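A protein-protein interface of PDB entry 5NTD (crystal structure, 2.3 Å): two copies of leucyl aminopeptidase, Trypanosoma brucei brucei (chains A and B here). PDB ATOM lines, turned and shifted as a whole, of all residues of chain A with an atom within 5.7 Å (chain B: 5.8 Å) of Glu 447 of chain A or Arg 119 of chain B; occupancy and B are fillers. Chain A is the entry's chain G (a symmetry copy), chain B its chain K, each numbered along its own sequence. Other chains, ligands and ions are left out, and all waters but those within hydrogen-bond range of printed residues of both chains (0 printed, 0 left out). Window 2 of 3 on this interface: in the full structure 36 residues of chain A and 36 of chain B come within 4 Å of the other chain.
The guanidinium group (NH2) of Arg 119 of chain B lies within hydrogen-bond range of the backbone carbonyl oxygen (O) of Lys 110 of chain B, 2.8 Å away. NH1 of Arg 119 of chain B is in salt-bridge range of OD2 of Asp 121 of chain B (2.9 Å). SG of Cys 445 of chain A sits at hydrogen-bond distance from OE2 of Glu 447 of chain A, 3.4 Å away. A ring nitrogen (NE2) of His 449 of chain A sits at hydrogen-bond distance from the backbone NH (N) of Cys 445 of chain A, at 3.1 Å.
Of the printed residues of chain B, Glu 447 of chain A touches Ala 111 (3.5 Å), Ser 112 (2.9 Å), Asn 115 (2.8 Å) and Arg 119 (3.7 Å). Arg 119 of chain B touches two residues of chain A. Printed residues of chain A within 4 Å of Asn 115 of chain B: Glu 447 and Tyr 448. Of the printed residues of chain B, Pro 446 of chain A touches Ser 112. Of the printed residues of chain A, Ala 111 of chain B touches Glu 447. Printed residues of chain A within 4 Å of Ser 112 of chain B: Cys 445, Pro 446 and Glu 447. Pro 120 of chain B touches none of the printed residues of chain A. Val 123 of chain B touches none of the printed residues of chain A. The nearest residue of chain B that does not touch Glu 447 of chain A is Lys 110 of chain B (4.6 Å). The nearest printed residue of chain A that does not touch Asn 115 of chain B is Cys 445 of chain A (4.04 Å).
No position is printed for both chains.
Printed residues of chain B that touch a printed residue of chain A: Ala 111, Ser 112, Asn 115, Arg 119 and Asp 121. Printed residues of chain A that touch a printed residue of chain B: Cys 445, Pro 446, Glu 447 and Tyr 448. Among the printed residues, no Asp or Glu carboxylate lies within 4 Å of a Lys or Arg side-chain nitrogen of the other chain.
Among the printed residues, merely in contact across the chains: Glu 447 of chain A with Ala 111 of chain B (3.5 Å), Glu 447 of chain A with Arg 119 of chain B (3.7 Å), Pro 446 of chain A with Ser 112 of chain B (3.9 Å) and Tyr 448 of chain A with Arg 119 of chain B (3.98 Å).
OG of Ser 112 of chain B lies close to SG of Cys 445 of chain A, 3.7 Å away. OE2 of Glu 447 of chain A is in hydrogen-bond range of N of Ser 112 of chain B, at 2.9 Å. The side-chain amide nitrogen (ND2) of Asn 115 of chain B sits at hydrogen-bond distance from the side-chain carboxylate (OE2) of Glu 447 of chain A (2.8 Å). The side-chain hydroxyl (OH) of Tyr 448 of chain A is in hydrogen-bond range of the side-chain amide nitrogen (ND2) of Asn 115 of chain B. OD1 of Asp 121 of chain B sits close to OH of Tyr 448 of chain A, at 3.5 Å.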
ATOM      1  N   CYS A 445     -28.662  -2.554 -17.990  1.00  0.00           N
ATOM      2  CA  CYS A 445     -28.668  -2.660 -16.511  1.00  0.00           C
ATOM      3  C   CYS A 445     -27.833  -3.854 -16.032  1.00  0.00           C
ATOM      4  O   CYS A 445     -28.367  -4.821 -15.498  1.00  0.00           O
ATOM      5  CB  CYS A 445     -30.090  -2.744 -15.991  1.00  0.00           C
ATOM      6  SG  CYS A 445     -30.176  -2.351 -14.231  1.00  0.00           S
ATOM      7  N   PRO A 446     -26.508  -3.806 -16.256  1.00  0.00           N
ATOM      8  CA  PRO A 446     -25.594  -4.896 -15.918  1.00  0.00           C
ATOM      9  C   PRO A 446     -25.755  -5.460 -14.513  1.00  0.00           C
ATOM     10  O   PRO A 446     -25.580  -6.635 -14.309  1.00  0.00           O
ATOM     11  CB  PRO A 446     -24.196  -4.249 -16.038  1.00  0.00           C
ATOM     12  CG  PRO A 446     -24.369  -3.035 -16.816  1.00  0.00           C
ATOM     13  CD  PRO A 446     -25.797  -2.595 -16.681  1.00  0.00           C
ATOM     14  N   GLU A 447     -26.036  -4.611 -13.553  1.00  0.00           N
ATOM     15  CA  GLU A 447     -26.213  -5.077 -12.166  1.00  0.00           C
ATOM     16  C   GLU A 447     -27.356  -6.084 -12.032  1.00  0.00           C
ATOM     17  O   GLU A 447     -27.340  -6.928 -11.167  1.00  0.00           O
ATOM     18  CB  GLU A 447     -26.389  -3.916 -11.167  1.00  0.00           C
ATOM     19  CG  GLU A 447     -27.610  -3.021 -11.397  1.00  0.00           C
ATOM     20  CD  GLU A 447     -27.341  -1.815 -12.272  1.00  0.00           C
ATOM     21  OE1 GLU A 447     -26.499  -1.898 -13.198  1.00  0.00           O
ATOM     22  OE2 GLU A 447     -28.023  -0.775 -12.058  1.00  0.00           O
ATOM     23  N   TYR A 448     -28.336  -6.002 -12.916  1.00  0.00           N
ATOM     24  CA  TYR A 448     -29.438  -6.999 -12.957  1.00  0.00           C
ATOM     25  C   TYR A 448     -29.209  -8.173 -13.910  1.00  0.00           C
ATOM     26  O   TYR A 448     -29.806  -9.219 -13.747  1.00  0.00           O
ATOM     27  CB  TYR A 448     -30.782  -6.336 -13.286  1.00  0.00           C
ATOM     28  CG  TYR A 448     -31.281  -5.341 -12.273  1.00  0.00           C
ATOM     29  CD1 TYR A 448     -30.748  -5.282 -10.957  1.00  0.00           C
ATOM     30  CD2 TYR A 448     -32.329  -4.483 -12.590  1.00  0.00           C
ATOM     31  CE1 TYR A 448     -31.231  -4.366 -10.026  1.00  0.00           C
ATOM     32  CE2 TYR A 448     -32.820  -3.587 -11.655  1.00  0.00           C
ATOM     33  CZ  TYR A 448     -32.258  -3.518 -10.375  1.00  0.00           C
ATOM     34  OH  TYR A 448     -32.744  -2.622  -9.456  1.00  0.00           O
ATOM     35  N   HIS A 449     -28.357  -7.995 -14.901  1.00  0.00           N
ATOM     36  CA  HIS A 449     -28.019  -9.091 -15.855  1.00  0.00           C
ATOM     37  C   HIS A 449     -27.011 -10.070 -15.275  1.00  0.00           C
ATOM     38  O   HIS A 449     -27.085 -11.265 -15.477  1.00  0.00           O
ATOM     39  CB  HIS A 449     -27.453  -8.569 -17.159  1.00  0.00           C
ATOM     40  CG  HIS A 449     -28.215  -7.429 -17.724  1.00  0.00           C
ATOM     41  ND1 HIS A 449     -29.586  -7.317 -17.606  1.00  0.00           N
ATOM     42  CD2 HIS A 449     -27.804  -6.316 -18.387  1.00  0.00           C
ATOM     43  CE1 HIS A 449     -29.988  -6.197 -18.176  1.00  0.00           C
ATOM     44  NE2 HIS A 449     -28.929  -5.559 -18.635  1.00  0.00           N
ATOM     45  N   GLU A 450     -26.039  -9.518 -14.588  1.00  0.00           N
ATOM     46  CA  GLU A 450     -24.898 -10.277 -14.046  1.00  0.00           C
ATOM     47  C   GLU A 450     -25.276 -11.541 -13.238  1.00  0.00           C
ATOM     48  O   GLU A 450     -24.715 -12.591 -13.477  1.00  0.00           O
ATOM     49  CB  GLU A 450     -24.034  -9.351 -13.205  1.00  0.00           C
ATOM     50  CG  GLU A 450     -22.794  -9.977 -12.626  1.00  0.00           C
ATOM     51  CD  GLU A 450     -22.072  -9.015 -11.704  1.00  0.00           C
ATOM     52  OE1 GLU A 450     -22.472  -7.809 -11.582  1.00  0.00           O
ATOM     53  OE2 GLU A 450     -21.088  -9.497 -11.074  1.00  0.00           O
ATOM     54  N   PRO A 451     -26.215 -11.436 -12.298  1.00  0.00           N
ATOM     55  CA  PRO A 451     -26.578 -12.620 -11.492  1.00  0.00           C
ATOM     56  C   PRO A 451     -27.161 -13.784 -12.284  1.00  0.00           C
ATOM     57  O   PRO A 451     -27.113 -14.927 -11.827  1.00  0.00           O
ATOM     58  CB  PRO A 451     -27.635 -12.087 -10.518  1.00  0.00           C
ATOM     59  CG  PRO A 451     -27.542 -10.605 -10.588  1.00  0.00           C
ATOM     60  CD  PRO A 451     -27.034 -10.274 -11.951  1.00  0.00           C
ATOM     61  N   VAL B 107     -25.032  -1.727   0.890  1.00  0.00           N
ATOM     62  CA  VAL B 107     -25.688  -1.392  -0.355  1.00  0.00           C
ATOM     63  C   VAL B 107     -24.651  -1.018  -1.425  1.00  0.00           C
ATOM     64  O   VAL B 107     -23.766  -0.207  -1.171  1.00  0.00           O
ATOM     65  CB  VAL B 107     -26.614  -0.183  -0.182  1.00  0.00           C
ATOM     66  CG1 VAL B 107     -27.394   0.098  -1.475  1.00  0.00           C
ATOM     67  CG2 VAL B 107     -27.575  -0.401   0.977  1.00  0.00           C
ATOM     68  N   PRO B 108     -24.760  -1.573  -2.640  1.00  0.00           N
ATOM     69  CA  PRO B 108     -23.824  -1.185  -3.672  1.00  0.00           C
ATOM     70  C   PRO B 108     -24.044   0.238  -4.112  1.00  0.00           C
ATOM     71  O   PRO B 108     -25.127   0.795  -3.953  1.00  0.00           O
ATOM     72  CB  PRO B 108     -24.141  -2.142  -4.821  1.00  0.00           C
ATOM     73  CG  PRO B 108     -25.542  -2.536  -4.606  1.00  0.00           C
ATOM     74  CD  PRO B 108     -25.685  -2.608  -3.108  1.00  0.00           C
ATOM     75  N   THR B 109     -22.987   0.848  -4.623  1.00  0.00           N
ATOM     76  CA  THR B 109     -23.113   2.180  -5.234  1.00  0.00           C
ATOM     77  C   THR B 109     -23.318   2.051  -6.757  1.00  0.00           C
ATOM     78  O   THR B 109     -23.800   2.978  -7.365  1.00  0.00           O
ATOM     79  CB  THR B 109     -21.908   3.132  -5.023  1.00  0.00           C
ATOM     80  OG1 THR B 109     -20.723   2.472  -5.434  1.00  0.00           O
ATOM     81  CG2 THR B 109     -21.807   3.607  -3.593  1.00  0.00           C
ATOM     82  N   LYS B 110     -22.867   0.947  -7.348  1.00  0.00           N
ATOM     83  CA  LYS B 110     -23.055   0.654  -8.782  1.00  0.00           C
ATOM     84  C   LYS B 110     -24.539   0.809  -9.114  1.00  0.00           C
ATOM     85  O   LYS B 110     -25.405   0.272  -8.434  1.00  0.00           O
ATOM     86  CB  LYS B 110     -22.587  -0.780  -9.159  1.00  0.00           C
ATOM     87  N   ALA B 111     -24.812   1.600 -10.127  1.00  0.00           N
ATOM     88  CA  ALA B 111     -26.175   1.826 -10.608  1.00  0.00           C
ATOM     89  C   ALA B 111     -26.133   2.385 -12.018  1.00  0.00           C
ATOM     90  O   ALA B 111     -25.617   3.447 -12.224  1.00  0.00           O
ATOM     91  CB  ALA B 111     -26.914   2.794  -9.699  1.00  0.00           C
ATOM     92  N   SER B 112     -26.683   1.655 -12.971  1.00  0.00           N
ATOM     93  CA  SER B 112     -26.679   2.022 -14.383  1.00  0.00           C
ATOM     94  C   SER B 112     -27.617   3.197 -14.561  1.00  0.00           C
ATOM     95  O   SER B 112     -28.452   3.489 -13.724  1.00  0.00           O
ATOM     96  CB  SER B 112     -27.145   0.825 -15.276  1.00  0.00           C
ATOM     97  OG  SER B 112     -28.600   0.766 -15.500  1.00  0.00           O
ATOM     98  N   ASN B 115     -31.327   2.871 -13.715  1.00  0.00           N
ATOM     99  CA  ASN B 115     -31.609   2.429 -12.345  1.00  0.00           C
ATOM    100  C   ASN B 115     -31.667   3.562 -11.360  1.00  0.00           C
ATOM    101  O   ASN B 115     -31.358   4.694 -11.695  1.00  0.00           O
ATOM    102  CB  ASN B 115     -30.585   1.386 -11.896  1.00  0.00           C
ATOM    103  CG  ASN B 115     -31.143   0.381 -10.891  1.00  0.00           C
ATOM    104  OD1 ASN B 115     -32.248   0.538 -10.366  1.00  0.00           O
ATOM    105  ND2 ASN B 115     -30.344  -0.625 -10.579  1.00  0.00           N
ATOM    106  N   CYS B 116     -32.187   3.253 -10.182  1.00  0.00           N
ATOM    107  CA  CYS B 116     -32.286   4.209  -9.070  1.00  0.00           C
ATOM    108  C   CYS B 116     -30.959   4.206  -8.341  1.00  0.00           C
ATOM    109  O   CYS B 116     -30.534   3.150  -7.892  1.00  0.00           O
ATOM    110  CB  CYS B 116     -33.388   3.813  -8.108  1.00  0.00           C
ATOM    111  SG  CYS B 116     -33.449   4.833  -6.614  1.00  0.00           S
ATOM    112  N   PRO B 117     -30.265   5.366  -8.277  1.00  0.00           N
ATOM    113  CA  PRO B 117     -28.896   5.427  -7.687  1.00  0.00           C
ATOM    114  C   PRO B 117     -28.788   4.930  -6.241  1.00  0.00           C
ATOM    115  O   PRO B 117     -27.772   4.375  -5.868  1.00  0.00           O
ATOM    116  CB  PRO B 117     -28.557   6.915  -7.729  1.00  0.00           C
ATOM    117  CG  PRO B 117     -29.383   7.467  -8.844  1.00  0.00           C
ATOM    118  CD  PRO B 117     -30.645   6.654  -8.887  1.00  0.00           C
ATOM    119  N   ALA B 118     -29.879   5.066  -5.492  1.00  0.00           N
ATOM    120  CA  ALA B 118     -29.931   4.593  -4.108  1.00  0.00           C
ATOM    121  C   ALA B 118     -30.066   3.086  -3.975  1.00  0.00           C
ATOM    122  O   ALA B 118     -30.003   2.540  -2.874  1.00  0.00           O
ATOM    123  CB  ALA B 118     -31.053   5.268  -3.375  1.00  0.00           C
ATOM    124  N   ARG B 119     -30.237   2.413  -5.088  1.00  0.00           N
ATOM    125  CA  ARG B 119     -30.358   0.929  -5.127  1.00  0.00           C
ATOM    126  C   ARG B 119     -31.299   0.363  -4.037  1.00  0.00           C
ATOM    127  O   ARG B 119     -30.912  -0.481  -3.249  1.00  0.00           O
ATOM    128  CB  ARG B 119     -28.996   0.268  -5.047  1.00  0.00           C
ATOM    129  CG  ARG B 119     -28.124   0.579  -6.252  1.00  0.00           C
ATOM    130  CD  ARG B 119     -28.640  -0.028  -7.554  1.00  0.00           C
ATOM    131  NE  ARG B 119     -28.884  -1.471  -7.408  1.00  0.00           N
ATOM    132  CZ  ARG B 119     -27.981  -2.435  -7.592  1.00  0.00           C
ATOM    133  NH1 ARG B 119     -28.327  -3.682  -7.398  1.00  0.00           N
ATOM    134  NH2 ARG B 119     -26.730  -2.153  -7.955  1.00  0.00           N
ATOM    135  N   PRO B 120     -32.537   0.855  -4.002  1.00  0.00           N
ATOM    136  CA  PRO B 120     -33.503   0.363  -3.043  1.00  0.00           C
ATOM    137  C   PRO B 120     -33.798  -1.116  -3.177  1.00  0.00           C
ATOM    138  O   PRO B 120     -34.309  -1.728  -2.265  1.00  0.00           O
ATOM    139  CB  PRO B 120     -34.744   1.212  -3.354  1.00  0.00           C
ATOM    140  CG  PRO B 120     -34.579   1.638  -4.777  1.00  0.00           C
ATOM    141  CD  PRO B 120     -33.114   1.874  -4.897  1.00  0.00           C
ATOM    142  N   ASP B 121     -33.528  -1.671  -4.348  1.00  0.00           N
ATOM    143  CA  ASP B 121     -33.690  -3.108  -4.573  1.00  0.00           C
ATOM    144  C   ASP B 121     -32.874  -3.875  -3.554  1.00  0.00           C
ATOM    145  O   ASP B 121     -33.325  -4.870  -2.994  1.00  0.00           O
ATOM    146  CB  ASP B 121     -33.293  -3.528  -5.993  1.00  0.00           C
ATOM    147  CG  ASP B 121     -31.867  -3.163  -6.342  1.00  0.00           C
ATOM    148  OD1 ASP B 121     -31.519  -1.958  -6.298  1.00  0.00           O
ATOM    149  OD2 ASP B 121     -31.090  -4.074  -6.659  1.00  0.00           O
ATOM    150  N   VAL B 122     -31.649  -3.431  -3.339  1.00  0.00           N
ATOM    151  CA  VAL B 122     -30.755  -4.115  -2.391  1.00  0.00           C
ATOM    152  C   VAL B 122     -31.144  -3.791  -0.942  1.00  0.00           C
ATOM    153  O   VAL B 122     -31.094  -4.634  -0.076  1.00  0.00           O
ATOM    154  CB  VAL B 122     -29.293  -3.778  -2.638  1.00  0.00           C
ATOM    155  CG1 VAL B 122     -28.407  -4.444  -1.575  1.00  0.00           C
ATOM    156  CG2 VAL B 122     -28.890  -4.275  -4.009  1.00  0.00           C
ATOM    157  N   VAL B 123     -31.545  -2.560  -0.714  1.00  0.00           N
ATOM    158  CA  VAL B 123     -32.039  -2.150   0.611  1.00  0.00           C
ATOM    159  C   VAL B 123     -33.113  -3.147   1.059  1.00  0.00           C
ATOM    160  O   VAL B 123     -33.074  -3.672   2.165  1.00  0.00           O
ATOM    161  CB  VAL B 123     -32.593  -0.702   0.631  1.00  0.00           C
ATOM    162  CG1 VAL B 123     -33.256  -0.369   1.967  1.00  0.00           C
ATOM    163  CG2 VAL B 123     -31.476   0.289   0.388  1.00  0.00           C
ATOM    164  N   THR B 124     -34.076  -3.388   0.184  1.00  0.00           N
ATOM    165  CA  THR B 124     -35.183  -4.316   0.476  1.00  0.00           C
ATOM    166  C   THR B 124     -34.636  -5.710   0.845  1.00  0.00           C
ATOM    167  O   THR B 124     -34.997  -6.288   1.853  1.00  0.00           O
ATOM    168  CB  THR B 124     -36.167  -4.439  -0.702  1.00  0.00           C
ATOM    169  OG1 THR B 124     -36.823  -3.182  -0.891  1.00  0.00           O
ATOM    170  CG2 THR B 124     -37.206  -5.518  -0.440  1.00  0.00           C
